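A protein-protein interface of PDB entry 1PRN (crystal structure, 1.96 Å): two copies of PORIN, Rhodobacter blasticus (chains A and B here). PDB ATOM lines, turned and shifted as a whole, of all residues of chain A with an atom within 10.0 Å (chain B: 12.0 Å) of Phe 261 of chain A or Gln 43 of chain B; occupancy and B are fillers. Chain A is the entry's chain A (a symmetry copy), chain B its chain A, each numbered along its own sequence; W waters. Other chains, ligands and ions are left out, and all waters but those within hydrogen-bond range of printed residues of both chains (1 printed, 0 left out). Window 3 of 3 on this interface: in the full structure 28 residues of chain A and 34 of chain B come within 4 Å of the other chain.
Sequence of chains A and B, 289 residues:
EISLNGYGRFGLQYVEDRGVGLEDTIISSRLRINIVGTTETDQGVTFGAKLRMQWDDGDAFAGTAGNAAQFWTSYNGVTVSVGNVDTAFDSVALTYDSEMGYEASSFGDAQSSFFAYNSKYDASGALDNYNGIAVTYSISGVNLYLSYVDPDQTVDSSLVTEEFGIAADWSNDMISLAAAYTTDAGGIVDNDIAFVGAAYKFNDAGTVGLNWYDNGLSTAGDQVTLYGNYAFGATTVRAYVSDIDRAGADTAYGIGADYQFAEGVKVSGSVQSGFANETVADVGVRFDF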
ATOM      1  N   GLY A 233      10.827  -8.708 -15.422  1.00  0.00           N
ATOM      2  CA  GLY A 233      10.422  -9.863 -16.208  1.00  0.00           C
ATOM      3  C   GLY A 233      11.570 -10.514 -16.962  1.00  0.00           C
ATOM      4  O   GLY A 233      12.423 -11.169 -16.351  1.00  0.00           O
ATOM      5  N   ALA A 234      11.598 -10.345 -18.284  1.00  0.00           N
ATOM      6  CA  ALA A 234      12.655 -10.928 -19.109  1.00  0.00           C
ATOM      7  C   ALA A 234      13.785  -9.944 -19.390  1.00  0.00           C
ATOM      8  O   ALA A 234      14.824 -10.333 -19.924  1.00  0.00           O
ATOM      9  CB  ALA A 234      12.085 -11.445 -20.427  1.00  0.00           C
ATOM     10  N   THR A 235      13.565  -8.669 -19.097  1.00  0.00           N
ATOM     11  CA  THR A 235      14.602  -7.686 -19.342  1.00  0.00           C
ATOM     12  C   THR A 235      15.229  -7.200 -18.050  1.00  0.00           C
ATOM     13  O   THR A 235      14.539  -7.017 -17.055  1.00  0.00           O
ATOM     14  CB  THR A 235      14.113  -6.525 -20.251  1.00  0.00           C
ATOM     15  OG1 THR A 235      14.415  -5.266 -19.646  1.00  0.00           O
ATOM     16  CG2 THR A 235      12.637  -6.637 -20.562  1.00  0.00           C
ATOM     17  N   THR A 236      16.554  -7.127 -18.035  1.00  0.00           N
ATOM     18  CA  THR A 236      17.286  -6.660 -16.871  1.00  0.00           C
ATOM     19  C   THR A 236      18.011  -5.377 -17.243  1.00  0.00           C
ATOM     20  O   THR A 236      18.540  -5.264 -18.345  1.00  0.00           O
ATOM     21  CB  THR A 236      18.320  -7.698 -16.414  1.00  0.00           C
ATOM     22  OG1 THR A 236      17.645  -8.915 -16.088  1.00  0.00           O
ATOM     23  CG2 THR A 236      19.079  -7.210 -15.187  1.00  0.00           C
ATOM     24  N   ASP A 258      19.721  -6.457 -20.593  1.00  0.00           N
ATOM     25  CA  ASP A 258      19.756  -7.834 -21.056  1.00  0.00           C
ATOM     26  C   ASP A 258      18.319  -8.229 -21.333  1.00  0.00           C
ATOM     27  O   ASP A 258      17.387  -7.741 -20.674  1.00  0.00           O
ATOM     28  CB  ASP A 258      20.286  -8.778 -19.982  1.00  0.00           C
ATOM     29  CG  ASP A 258      21.724  -8.524 -19.626  1.00  0.00           C
ATOM     30  OD1 ASP A 258      22.493  -8.057 -20.481  1.00  0.00           O
ATOM     31  OD2 ASP A 258      22.093  -8.823 -18.482  1.00  0.00           O
ATOM     32  N   TYR A 259      18.136  -9.107 -22.301  1.00  0.00           N
ATOM     33  CA  TYR A 259      16.818  -9.587 -22.621  1.00  0.00           C
ATOM     34  C   TYR A 259      16.907 -11.085 -22.819  1.00  0.00           C
ATOM     35  O   TYR A 259      17.574 -11.565 -23.736  1.00  0.00           O
ATOM     36  CB  TYR A 259      16.283  -8.916 -23.872  1.00  0.00           C
ATOM     37  CG  TYR A 259      14.898  -9.386 -24.179  1.00  0.00           C
ATOM     38  CD1 TYR A 259      13.839  -9.078 -23.324  1.00  0.00           C
ATOM     39  CD2 TYR A 259      14.643 -10.191 -25.280  1.00  0.00           C
ATOM     40  CE1 TYR A 259      12.560  -9.563 -23.551  1.00  0.00           C
ATOM     41  CE2 TYR A 259      13.367 -10.683 -25.523  1.00  0.00           C
ATOM     42  CZ  TYR A 259      12.328 -10.365 -24.651  1.00  0.00           C
ATOM     43  OH  TYR A 259      11.058 -10.847 -24.885  1.00  0.00           O
ATOM     44  N   GLN A 260      16.271 -11.826 -21.927  1.00  0.00           N
ATOM     45  CA  GLN A 260      16.280 -13.269 -22.013  1.00  0.00           C
ATOM     46  C   GLN A 260      15.256 -13.706 -23.050  1.00  0.00           C
ATOM     47  O   GLN A 260      14.075 -13.871 -22.748  1.00  0.00           O
ATOM     48  CB  GLN A 260      15.951 -13.876 -20.657  1.00  0.00           C
ATOM     49  CG  GLN A 260      16.349 -15.320 -20.531  1.00  0.00           C
ATOM     50  CD  GLN A 260      17.851 -15.508 -20.457  1.00  0.00           C
ATOM     51  OE1 GLN A 260      18.533 -14.820 -19.702  1.00  0.00           O
ATOM     52  NE2 GLN A 260      18.374 -16.432 -21.249  1.00  0.00           N
ATOM     53  N   PHE A 261      15.719 -13.876 -24.280  1.00  0.00           N
ATOM     54  CA  PHE A 261      14.869 -14.274 -25.394  1.00  0.00           C
ATOM     55  C   PHE A 261      14.261 -15.668 -25.212  1.00  0.00           C
ATOM     56  O   PHE A 261      13.107 -15.904 -25.566  1.00  0.00           O
ATOM     57  CB  PHE A 261      15.679 -14.197 -26.695  1.00  0.00           C
ATOM     58  CG  PHE A 261      14.922 -14.647 -27.922  1.00  0.00           C
ATOM     59  CD1 PHE A 261      13.940 -13.842 -28.489  1.00  0.00           C
ATOM     60  CD2 PHE A 261      15.193 -15.880 -28.510  1.00  0.00           C
ATOM     61  CE1 PHE A 261      13.240 -14.264 -29.626  1.00  0.00           C
ATOM     62  CE2 PHE A 261      14.499 -16.304 -29.640  1.00  0.00           C
ATOM     63  CZ  PHE A 261      13.523 -15.492 -30.198  1.00  0.00           C
ATOM     64  N   ALA A 262      15.056 -16.593 -24.696  1.00  0.00           N
ATOM     65  CA  ALA A 262      14.636 -17.967 -24.472  1.00  0.00           C
ATOM     66  C   ALA A 262      15.709 -18.553 -23.585  1.00  0.00           C
ATOM     67  O   ALA A 262      16.701 -17.888 -23.302  1.00  0.00           O
ATOM     68  CB  ALA A 262      14.568 -18.726 -25.797  1.00  0.00           C
ATOM     69  N   GLU A 263      15.521 -19.769 -23.098  1.00  0.00           N
ATOM     70  CA  GLU A 263      16.542 -20.369 -22.252  1.00  0.00           C
ATOM     71  C   GLU A 263      17.826 -20.515 -23.097  1.00  0.00           C
ATOM     72  O   GLU A 263      17.793 -21.044 -24.215  1.00  0.00           O
ATOM     73  CB  GLU A 263      16.091 -21.743 -21.731  1.00  0.00           C
ATOM     74  CG  GLU A 263      16.870 -22.194 -20.460  1.00  0.00           C
ATOM     75  CD  GLU A 263      17.184 -23.694 -20.431  1.00  0.00           C
ATOM     76  OE1 GLU A 263      16.243 -24.501 -20.223  1.00  0.00           O
ATOM     77  OE2 GLU A 263      18.378 -24.061 -20.601  1.00  0.00           O
ATOM     78  N   GLY A 264      18.943 -20.019 -22.588  1.00  0.00           N
ATOM     79  CA  GLY A 264      20.170 -20.132 -23.347  1.00  0.00           C
ATOM     80  C   GLY A 264      20.387 -19.089 -24.435  1.00  0.00           C
ATOM     81  O   GLY A 264      21.379 -19.185 -25.147  1.00  0.00           O
ATOM     82  N   VAL A 265      19.462 -18.147 -24.624  1.00  0.00           N
ATOM     83  CA  VAL A 265      19.616 -17.095 -25.632  1.00  0.00           C
ATOM     84  C   VAL A 265      19.412 -15.734 -24.974  1.00  0.00           C
ATOM     85  O   VAL A 265      18.294 -15.373 -24.594  1.00  0.00           O
ATOM     86  CB  VAL A 265      18.617 -17.218 -26.796  1.00  0.00           C
ATOM     87  CG1 VAL A 265      18.871 -16.110 -27.815  1.00  0.00           C
ATOM     88  CG2 VAL A 265      18.754 -18.566 -27.456  1.00  0.00           C
ATOM     89  N   LYS A 266      20.488 -14.962 -24.876  1.00  0.00           N
ATOM     90  CA  LYS A 266      20.422 -13.657 -24.236  1.00  0.00           C
ATOM     91  C   LYS A 266      20.854 -12.540 -25.174  1.00  0.00           C
ATOM     92  O   LYS A 266      21.913 -12.634 -25.788  1.00  0.00           O
ATOM     93  CB  LYS A 266      21.320 -13.675 -23.000  1.00  0.00           C
ATOM     94  CG  LYS A 266      21.335 -12.425 -22.215  1.00  0.00           C
ATOM     95  CD  LYS A 266      22.198 -13.127 -21.245  1.00  0.00           C
ATOM     96  CE  LYS A 266      22.847 -12.180 -20.315  1.00  0.00           C
ATOM     97  NZ  LYS A 266      23.667 -12.881 -19.279  1.00  0.00           N
ATOM     98  N   VAL A 267      19.999 -11.532 -25.341  1.00  0.00           N
ATOM     99  CA  VAL A 267      20.311 -10.370 -26.176  1.00  0.00           C
ATOM    100  C   VAL A 267      20.740  -9.277 -25.185  1.00  0.00           C
ATOM    101  O   VAL A 267      20.091  -9.100 -24.155  1.00  0.00           O
ATOM    102  CB  VAL A 267      19.090  -9.925 -26.985  1.00  0.00           C
ATOM    103  CG1 VAL A 267      19.441  -8.760 -27.874  1.00  0.00           C
ATOM    104  CG2 VAL A 267      18.615 -11.064 -27.826  1.00  0.00           C
ATOM    105  N   SER A 268      21.873  -8.616 -25.441  1.00  0.00           N
ATOM    106  CA  SER A 268      22.382  -7.585 -24.532  1.00  0.00           C
ATOM    107  C   SER A 268      22.994  -6.411 -25.267  1.00  0.00           C
ATOM    108  O   SER A 268      23.477  -6.561 -26.386  1.00  0.00           O
ATOM    109  CB  SER A 268      23.459  -8.153 -23.607  1.00  0.00           C
ATOM    110  OG  SER A 268      23.027  -9.327 -22.952  1.00  0.00           O
ATOM    111  N   GLY A 284      24.354  -7.279 -29.099  1.00  0.00           N
ATOM    112  CA  GLY A 284      24.491  -8.585 -29.707  1.00  0.00           C
ATOM    113  C   GLY A 284      23.741  -9.678 -28.977  1.00  0.00           C
ATOM    114  O   GLY A 284      22.937  -9.417 -28.091  1.00  0.00           O
ATOM    115  N   VAL A 285      23.991 -10.914 -29.379  1.00  0.00           N
ATOM    116  CA  VAL A 285      23.336 -12.072 -28.777  1.00  0.00           C
ATOM    117  C   VAL A 285      24.367 -13.080 -28.357  1.00  0.00           C
ATOM    118  O   VAL A 285      25.392 -13.224 -29.012  1.00  0.00           O
ATOM    119  CB  VAL A 285      22.526 -12.921 -29.800  1.00  0.00           C
ATOM    120  CG1 VAL A 285      21.219 -13.356 -29.206  1.00  0.00           C
ATOM    121  CG2 VAL A 285      22.395 -12.245 -31.146  1.00  0.00           C
ATOM    122  N   ARG A 286      24.038 -13.832 -27.320  1.00  0.00           N
ATOM    123  CA  ARG A 286      24.858 -14.934 -26.871  1.00  0.00           C
ATOM    124  C   ARG A 286      23.893 -16.116 -26.797  1.00  0.00           C
ATOM    125  O   ARG A 286      22.795 -15.994 -26.248  1.00  0.00           O
ATOM    126  CB  ARG A 286      25.447 -14.693 -25.485  1.00  0.00           C
ATOM    127  CG  ARG A 286      26.125 -15.931 -24.956  1.00  0.00           C
ATOM    128  CD  ARG A 286      26.653 -15.805 -23.619  1.00  0.00           C
ATOM    129  NE  ARG A 286      26.923 -17.115 -23.034  1.00  0.00           N
ATOM    130  CZ  ARG A 286      27.891 -17.341 -22.158  1.00  0.00           C
ATOM    131  NH1 ARG A 286      28.683 -16.344 -21.785  1.00  0.00           N
ATOM    132  NH2 ARG A 286      28.043 -18.544 -21.614  1.00  0.00           N
ATOM    133  N   PHE A 287      24.275 -17.237 -27.393  1.00  0.00           N
ATOM    134  CA  PHE A 287      23.462 -18.435 -27.342  1.00  0.00           C
ATOM    135  C   PHE A 287      24.335 -19.591 -26.848  1.00  0.00           C
ATOM    136  O   PHE A 287      25.466 -19.774 -27.301  1.00  0.00           O
ATOM    137  CB  PHE A 287      22.796 -18.714 -28.689  1.00  0.00           C
ATOM    138  CG  PHE A 287      23.746 -18.783 -29.853  1.00  0.00           C
ATOM    139  CD1 PHE A 287      24.125 -17.629 -30.527  1.00  0.00           C
ATOM    140  CD2 PHE A 287      24.215 -20.008 -30.313  1.00  0.00           C
ATOM    141  CE1 PHE A 287      24.950 -17.688 -31.647  1.00  0.00           C
ATOM    142  CE2 PHE A 287      25.038 -20.072 -31.430  1.00  0.00           C
ATOM    143  CZ  PHE A 287      25.403 -18.906 -32.097  1.00  0.00           C
ATOM    144  N   THR B  38      24.146 -25.995 -31.760  1.00  0.00           N
ATOM    145  CA  THR B  38      22.836 -25.395 -32.037  1.00  0.00           C
ATOM    146  C   THR B  38      21.984 -25.144 -30.802  1.00  0.00           C
ATOM    147  O   THR B  38      21.987 -25.923 -29.853  1.00  0.00           O
ATOM    148  CB  THR B  38      21.995 -26.247 -33.014  1.00  0.00           C
ATOM    149  OG1 THR B  38      21.843 -27.559 -32.483  1.00  0.00           O
ATOM    150  CG2 THR B  38      22.657 -26.353 -34.347  1.00  0.00           C
ATOM    151  N   THR B  39      21.272 -24.029 -30.824  1.00  0.00           N
ATOM    152  CA  THR B  39      20.379 -23.653 -29.755  1.00  0.00           C
ATOM    153  C   THR B  39      19.005 -23.425 -30.383  1.00  0.00           C
ATOM    154  O   THR B  39      18.825 -22.510 -31.181  1.00  0.00           O
ATOM    155  CB  THR B  39      20.834 -22.361 -29.069  1.00  0.00           C
ATOM    156  OG1 THR B  39      22.210 -22.489 -28.694  1.00  0.00           O
ATOM    157  CG2 THR B  39      19.998 -22.103 -27.829  1.00  0.00           C
ATOM    158  N   GLU B  40      18.094 -24.359 -30.134  1.00  0.00           N
ATOM    159  CA  GLU B  40      16.717 -24.281 -30.621  1.00  0.00           C
ATOM    160  C   GLU B  40      15.881 -23.579 -29.556  1.00  0.00           C
ATOM    161  O   GLU B  40      16.203 -23.650 -28.364  1.00  0.00           O
ATOM    162  CB  GLU B  40      16.167 -25.680 -30.858  1.00  0.00           C
ATOM    163  CG  GLU B  40      16.902 -26.447 -31.937  1.00  0.00           C
ATOM    164  CD  GLU B  40      16.533 -27.934 -31.977  1.00  0.00           C
ATOM    165  OE1 GLU B  40      15.819 -28.427 -31.063  1.00  0.00           O
ATOM    166  OE2 GLU B  40      16.979 -28.618 -32.930  1.00  0.00           O
ATOM    167  N   THR B  41      14.854 -22.853 -29.974  1.00  0.00           N
ATOM    168  CA  THR B  41      13.996 -22.154 -29.025  1.00  0.00           C
ATOM    169  C   THR B  41      12.536 -22.463 -29.346  1.00  0.00           C
ATOM    170  O   THR B  41      12.211 -22.856 -30.472  1.00  0.00           O
ATOM    171  CB  THR B  41      14.229 -20.619 -29.064  1.00  0.00           C
ATOM    172  OG1 THR B  41      13.868 -20.103 -30.352  1.00  0.00           O
ATOM    173  CG2 THR B  41      15.696 -20.284 -28.793  1.00  0.00           C
ATOM    174  N   ASP B  42      11.648 -22.286 -28.372  1.00  0.00           N
ATOM    175  CA  ASP B  42      10.231 -22.548 -28.616  1.00  0.00           C
ATOM    176  C   ASP B  42       9.562 -21.475 -29.465  1.00  0.00           C
ATOM    177  O   ASP B  42       8.426 -21.632 -29.886  1.00  0.00           O
ATOM    178  CB  ASP B  42       9.462 -22.793 -27.314  1.00  0.00           C
ATOM    179  CG  ASP B  42       9.689 -21.723 -26.266  1.00  0.00           C
ATOM    180  OD1 ASP B  42      10.130 -20.600 -26.574  1.00  0.00           O
ATOM    181  OD2 ASP B  42       9.418 -22.021 -25.095  1.00  0.00           O
ATOM    182  N   GLN B  43      10.286 -20.395 -29.732  1.00  0.00           N
ATOM    183  CA  GLN B  43       9.782 -19.306 -30.553  1.00  0.00           C
ATOM    184  C   GLN B  43       9.976 -19.665 -32.020  1.00  0.00           C
ATOM    185  O   GLN B  43       9.557 -18.925 -32.899  1.00  0.00           O
ATOM    186  CB  GLN B  43      10.548 -18.013 -30.254  1.00  0.00           C
ATOM    187  CG  GLN B  43      10.697 -17.666 -28.742  1.00  0.00           C
ATOM    188  CD  GLN B  43       9.346 -17.482 -28.055  1.00  0.00           C
ATOM    189  OE1 GLN B  43       8.373 -17.059 -28.683  1.00  0.00           O
ATOM    190  NE2 GLN B  43       9.281 -17.806 -26.762  1.00  0.00           N
ATOM    191  N   GLY B  44      10.671 -20.770 -32.285  1.00  0.00           N
ATOM    192  CA  GLY B  44      10.914 -21.191 -33.653  1.00  0.00           C
ATOM    193  C   GLY B  44      12.151 -20.585 -34.321  1.00  0.00           C
ATOM    194  O   GLY B  44      12.312 -20.681 -35.543  1.00  0.00           O
ATOM    195  N   VAL B  45      13.010 -19.941 -33.532  1.00  0.00           N
ATOM    196  CA  VAL B  45      14.239 -19.343 -34.053  1.00  0.00           C
ATOM    197  C   VAL B  45      15.368 -20.248 -33.612  1.00  0.00           C
ATOM    198  O   VAL B  45      15.468 -20.569 -32.441  1.00  0.00           O
ATOM    199  CB  VAL B  45      14.507 -17.956 -33.461  1.00  0.00           C
ATOM    200  CG1 VAL B  45      15.798 -17.376 -34.053  1.00  0.00           C
ATOM    201  CG2 VAL B  45      13.330 -17.039 -33.721  1.00  0.00           C
ATOM    202  N   THR B  46      16.193 -20.691 -34.547  1.00  0.00           N
ATOM    203  CA  THR B  46      17.314 -21.560 -34.230  1.00  0.00           C
ATOM    204  C   THR B  46      18.606 -20.778 -34.398  1.00  0.00           C
ATOM    205  O   THR B  46      18.740 -20.009 -35.347  1.00  0.00           O
ATOM    206  CB  THR B  46      17.373 -22.762 -35.181  1.00  0.00           C
ATOM    207  OG1 THR B  46      16.191 -23.554 -35.031  1.00  0.00           O
ATOM    208  CG2 THR B  46      18.597 -23.629 -34.887  1.00  0.00           C
ATOM    209  N   PHE B  47      19.537 -20.963 -33.466  1.00  0.00           N
ATOM    210  CA  PHE B  47      20.849 -20.323 -33.513  1.00  0.00           C
ATOM    211  C   PHE B  47      21.880 -21.415 -33.676  1.00  0.00           C
ATOM    212  O   PHE B  47      21.718 -22.508 -33.141  1.00  0.00           O
ATOM    213  CB  PHE B  47      21.136 -19.561 -32.227  1.00  0.00           C
ATOM    214  CG  PHE B  47      20.249 -18.376 -32.031  1.00  0.00           C
ATOM    215  CD1 PHE B  47      18.994 -18.519 -31.433  1.00  0.00           C
ATOM    216  CD2 PHE B  47      20.653 -17.109 -32.458  1.00  0.00           C
ATOM    217  CE1 PHE B  47      18.144 -17.418 -31.280  1.00  0.00           C
ATOM    218  CE2 PHE B  47      19.813 -16.000 -32.308  1.00  0.00           C
ATOM    219  CZ  PHE B  47      18.555 -16.158 -31.712  1.00  0.00           C
ATOM    220  N   GLY B  48      22.932 -21.134 -34.426  1.00  0.00           N
ATOM    221  CA  GLY B  48      23.958 -22.130 -34.606  1.00  0.00           C
ATOM    222  C   GLY B  48      25.325 -21.540 -34.883  1.00  0.00           C
ATOM    223  O   GLY B  48      25.459 -20.368 -35.231  1.00  0.00           O
ATOM    224  N   TRP B  72      24.858 -18.441 -37.362  1.00  0.00           N
ATOM    225  CA  TRP B  72      23.638 -18.206 -38.121  1.00  0.00           C
ATOM    226  C   TRP B  72      22.400 -18.210 -37.250  1.00  0.00           C
ATOM    227  O   TRP B  72      22.418 -18.705 -36.114  1.00  0.00           O
ATOM    228  CB  TRP B  72      23.470 -19.228 -39.247  1.00  0.00           C
ATOM    229  CG  TRP B  72      23.191 -20.599 -38.758  1.00  0.00           C
ATOM    230  CD1 TRP B  72      21.972 -21.122 -38.398  1.00  0.00           C
ATOM    231  CD2 TRP B  72      24.153 -21.634 -38.537  1.00  0.00           C
ATOM    232  NE1 TRP B  72      22.124 -22.421 -37.969  1.00  0.00           N
ATOM    233  CE2 TRP B  72      23.457 -22.766 -38.054  1.00  0.00           C
ATOM    234  CE3 TRP B  72      25.543 -21.721 -38.713  1.00  0.00           C
ATOM    235  CZ2 TRP B  72      24.098 -23.967 -37.734  1.00  0.00           C
ATOM    236  CZ3 TRP B  72      26.185 -22.915 -38.400  1.00  0.00           C
ATOM    237  CH2 TRP B  72      25.460 -24.022 -37.914  1.00  0.00           C
ATOM    238  N   THR B  73      21.330 -17.666 -37.821  1.00  0.00           N
ATOM    239  CA  THR B  73      20.021 -17.574 -37.196  1.00  0.00           C
ATOM    240  C   THR B  73      19.024 -17.926 -38.291  1.00  0.00           C
ATOM    241  O   THR B  73      19.053 -17.322 -39.364  1.00  0.00           O
ATOM    242  CB  THR B  73      19.724 -16.134 -36.745  1.00  0.00           C
ATOM    243  OG1 THR B  73      20.796 -15.663 -35.931  1.00  0.00           O
ATOM    244  CG2 THR B  73      18.465 -16.090 -35.939  1.00  0.00           C
ATOM    245  N   SER B  74      18.176 -18.916 -38.027  1.00  0.00           N
ATOM    246  CA  SER B  74      17.155 -19.350 -38.978  1.00  0.00           C
ATOM    247  C   SER B  74      15.786 -19.167 -38.378  1.00  0.00           C
ATOM    248  O   SER B  74      15.574 -19.409 -37.190  1.00  0.00           O
ATOM    249  CB  SER B  74      17.303 -20.826 -39.321  1.00  0.00           C
ATOM    250  OG  SER B  74      18.615 -21.121 -39.700  1.00  0.00           O
ATOM    251  N   TYR B  75      14.848 -18.759 -39.216  1.00  0.00           N
ATOM    252  CA  TYR B  75      13.487 -18.554 -38.792  1.00  0.00           C
ATOM    253  C   TYR B  75      12.628 -18.528 -40.028  1.00  0.00           C
ATOM    254  O   TYR B  75      12.869 -17.744 -40.933  1.00  0.00           O
ATOM    255  CB  TYR B  75      13.351 -17.223 -38.073  1.00  0.00           C
ATOM    256  CG  TYR B  75      11.932 -16.923 -37.648  1.00  0.00           C
ATOM    257  CD1 TYR B  75      11.251 -17.778 -36.778  1.00  0.00           C
ATOM    258  CD2 TYR B  75      11.264 -15.787 -38.119  1.00  0.00           C
ATOM    259  CE1 TYR B  75       9.942 -17.505 -36.381  1.00  0.00           C
ATOM    260  CE2 TYR B  75       9.950 -15.503 -37.725  1.00  0.00           C
ATOM    261  CZ  TYR B  75       9.294 -16.368 -36.858  1.00  0.00           C
ATOM    262  OH  TYR B  75       8.003 -16.088 -36.453  1.00  0.00           O
ATOM    263  N   ASN B  76      11.671 -19.438 -40.096  1.00  0.00           N
ATOM    264  CA  ASN B  76      10.748 -19.495 -41.222  1.00  0.00           C
ATOM    265  C   ASN B  76      11.373 -19.606 -42.605  1.00  0.00           C
ATOM    266  O   ASN B  76      10.938 -18.923 -43.537  1.00  0.00           O
ATOM    267  CB  ASN B  76       9.821 -18.275 -41.194  1.00  0.00           C
ATOM    268  CG  ASN B  76       8.438 -18.611 -40.695  1.00  0.00           C
ATOM    269  OD1 ASN B  76       8.235 -18.855 -39.499  1.00  0.00           O
ATOM    270  ND2 ASN B  76       7.476 -18.665 -41.615  1.00  0.00           N
ATOM    271  N   GLY B  77      12.379 -20.459 -42.749  1.00  0.00           N
ATOM    272  CA  GLY B  77      13.005 -20.627 -44.047  1.00  0.00           C
ATOM    273  C   GLY B  77      14.057 -19.601 -44.408  1.00  0.00           C
ATOM    274  O   GLY B  77      14.688 -19.730 -45.449  1.00  0.00           O
ATOM    275  N   VAL B  78      14.224 -18.573 -43.583  1.00  0.00           N
ATOM    276  CA  VAL B  78      15.226 -17.542 -43.826  1.00  0.00           C
ATOM    277  C   VAL B  78      16.403 -17.796 -42.880  1.00  0.00           C
ATOM    278  O   VAL B  78      16.211 -18.109 -41.706  1.00  0.00           O
ATOM    279  CB  VAL B  78      14.676 -16.124 -43.540  1.00  0.00           C
ATOM    280  CG1 VAL B  78      15.746 -15.081 -43.789  1.00  0.00           C
ATOM    281  CG2 VAL B  78      13.467 -15.846 -44.410  1.00  0.00           C
HETATM  282  O   HOH W   1      15.843 -22.405 -25.903  1.00  0.00           O
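OD1 of Asp 42 of chain B sits at hydrogen-bond distance from NE2 of Gln 43 of chain B, at 2.9 Å. The side-chain amide nitrogen of Gln 260 of chain A sits at hydrogen-bond distance from the backbone carbonyl oxygen of Ala 262 of chain A, 3.0 Å away. The backbone NH (N) of Thr 39 of chain B is in hydrogen-bond range of the backbone carbonyl oxygen (O) of Phe 47 of chain B, at 2.8 Å. OG1 of Thr 41 of chain B lies within hydrogen-bond range of O of Val 45 of chain B. The backbone carbonyl oxygen of Gly 48 of chain B sits at hydrogen-bond distance from the backbone NH of Trp 72 of chain B, at 2.9 Å.
Phe 261 of chain A touches Thr 41 of chain B. CZ of Phe 261 of chain A touches CG of Gln 43 of chain B, at 3.9 Å. Phe 261 of chain A touches Val 45 of chain B (CZ to CG2, 3.9 Å). CG2 of Thr 41 of chain B touches CB of Ala 262 of chain A, at 3.6 Å. CG2 of Val 265 of chain A touches CG2 of Thr 39 of chain B, 3.8 Å away. Thr 41 of chain B touches Val 265 of chain A (CG2 to CG2, 3.8 Å). Val 265 of chain A touches Phe 47 of chain B. Phe 287 of chain A touches Thr 39 of chain B. CB of Phe 47 of chain B touches CG of Phe 287 of chain A (3.6 Å). O of Gly 48 of chain B touches CZ of Phe 287 of chain A, at 3.5 Å.
No residue of chain B comes within 4 Å of Gln 260 of chain A. Of chain B, only Thr 41 (3.9 Å), Gln 43 (3.9 Å) and Val 45 (3.9 Å) come within 4 Å of Phe 261 of chain A. Lys 266 of chain A touches none of the printed residues of chain B. No residue of chain B comes within 4 Å of Val 267 of chain A. Printed residues of chain B within 4 Å of Phe 287 of chain A: Thr 39 (3.6 Å), Phe 47 (3.6 Å) and Gly 48 (3.5 Å). Printed residues of chain A within 4 Å of Thr 39 of chain B: Val 265 (3.8 Å) and Phe 287 (3.6 Å). Glu 40 of chain B touches none of the printed residues of chain A. Printed residues of chain A within 4 Å of Thr 41 of chain B: Phe 261 (3.9 Å), Ala 262 (3.6 Å) and Val 265 (3.8 Å). No residue of chain A comes within 4 Å of Asp 42 of chain B. Gln 43 of chain B touches just one residue of chain A: Phe 261. No residue of chain A comes within 4 Å of Gly 44 of chain B. Of the printed residues of chain A, Phe 47 of chain B touches Val 265 and Phe 287. Printed residues of chain A within 4 Å of Gly 48 of chain B: Phe 287. The nearest residue of chain B that does not touch Phe 261 of chain A is Phe 47 of chain B (4.1 Å). The nearest residue of chain A that does not touch Gln 43 of chain B is Ala 262 of chain A (5.0 Å).
Of the 18 printed residues of chain B, 6 touch a printed residue of chain A. Printed residues of chain B that touch a printed residue of chain A: Thr 39, Thr 41, Gln 43, Val 45, Phe 47 and Gly 48. Of the 19 printed residues of chain A, 4 touch a printed residue of chain B. Hydrophobic or aromatic side chains of chain A within 4 Å of the printed part of chain B: Phe 261, Ala 262, Val 265 and Phe 287. Among the printed residues, 10 pairs touch across the chains.
No position is printed for both chains. Of the 10 pairs that touch across the chains among the printed residues, none has its exchanged pair printed and touching as well.
Water W1 bridges the backbone carbonyl oxygen of Glu 40 of chain B and the backbone carbonyl oxygen of Glu 263 of chain A.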
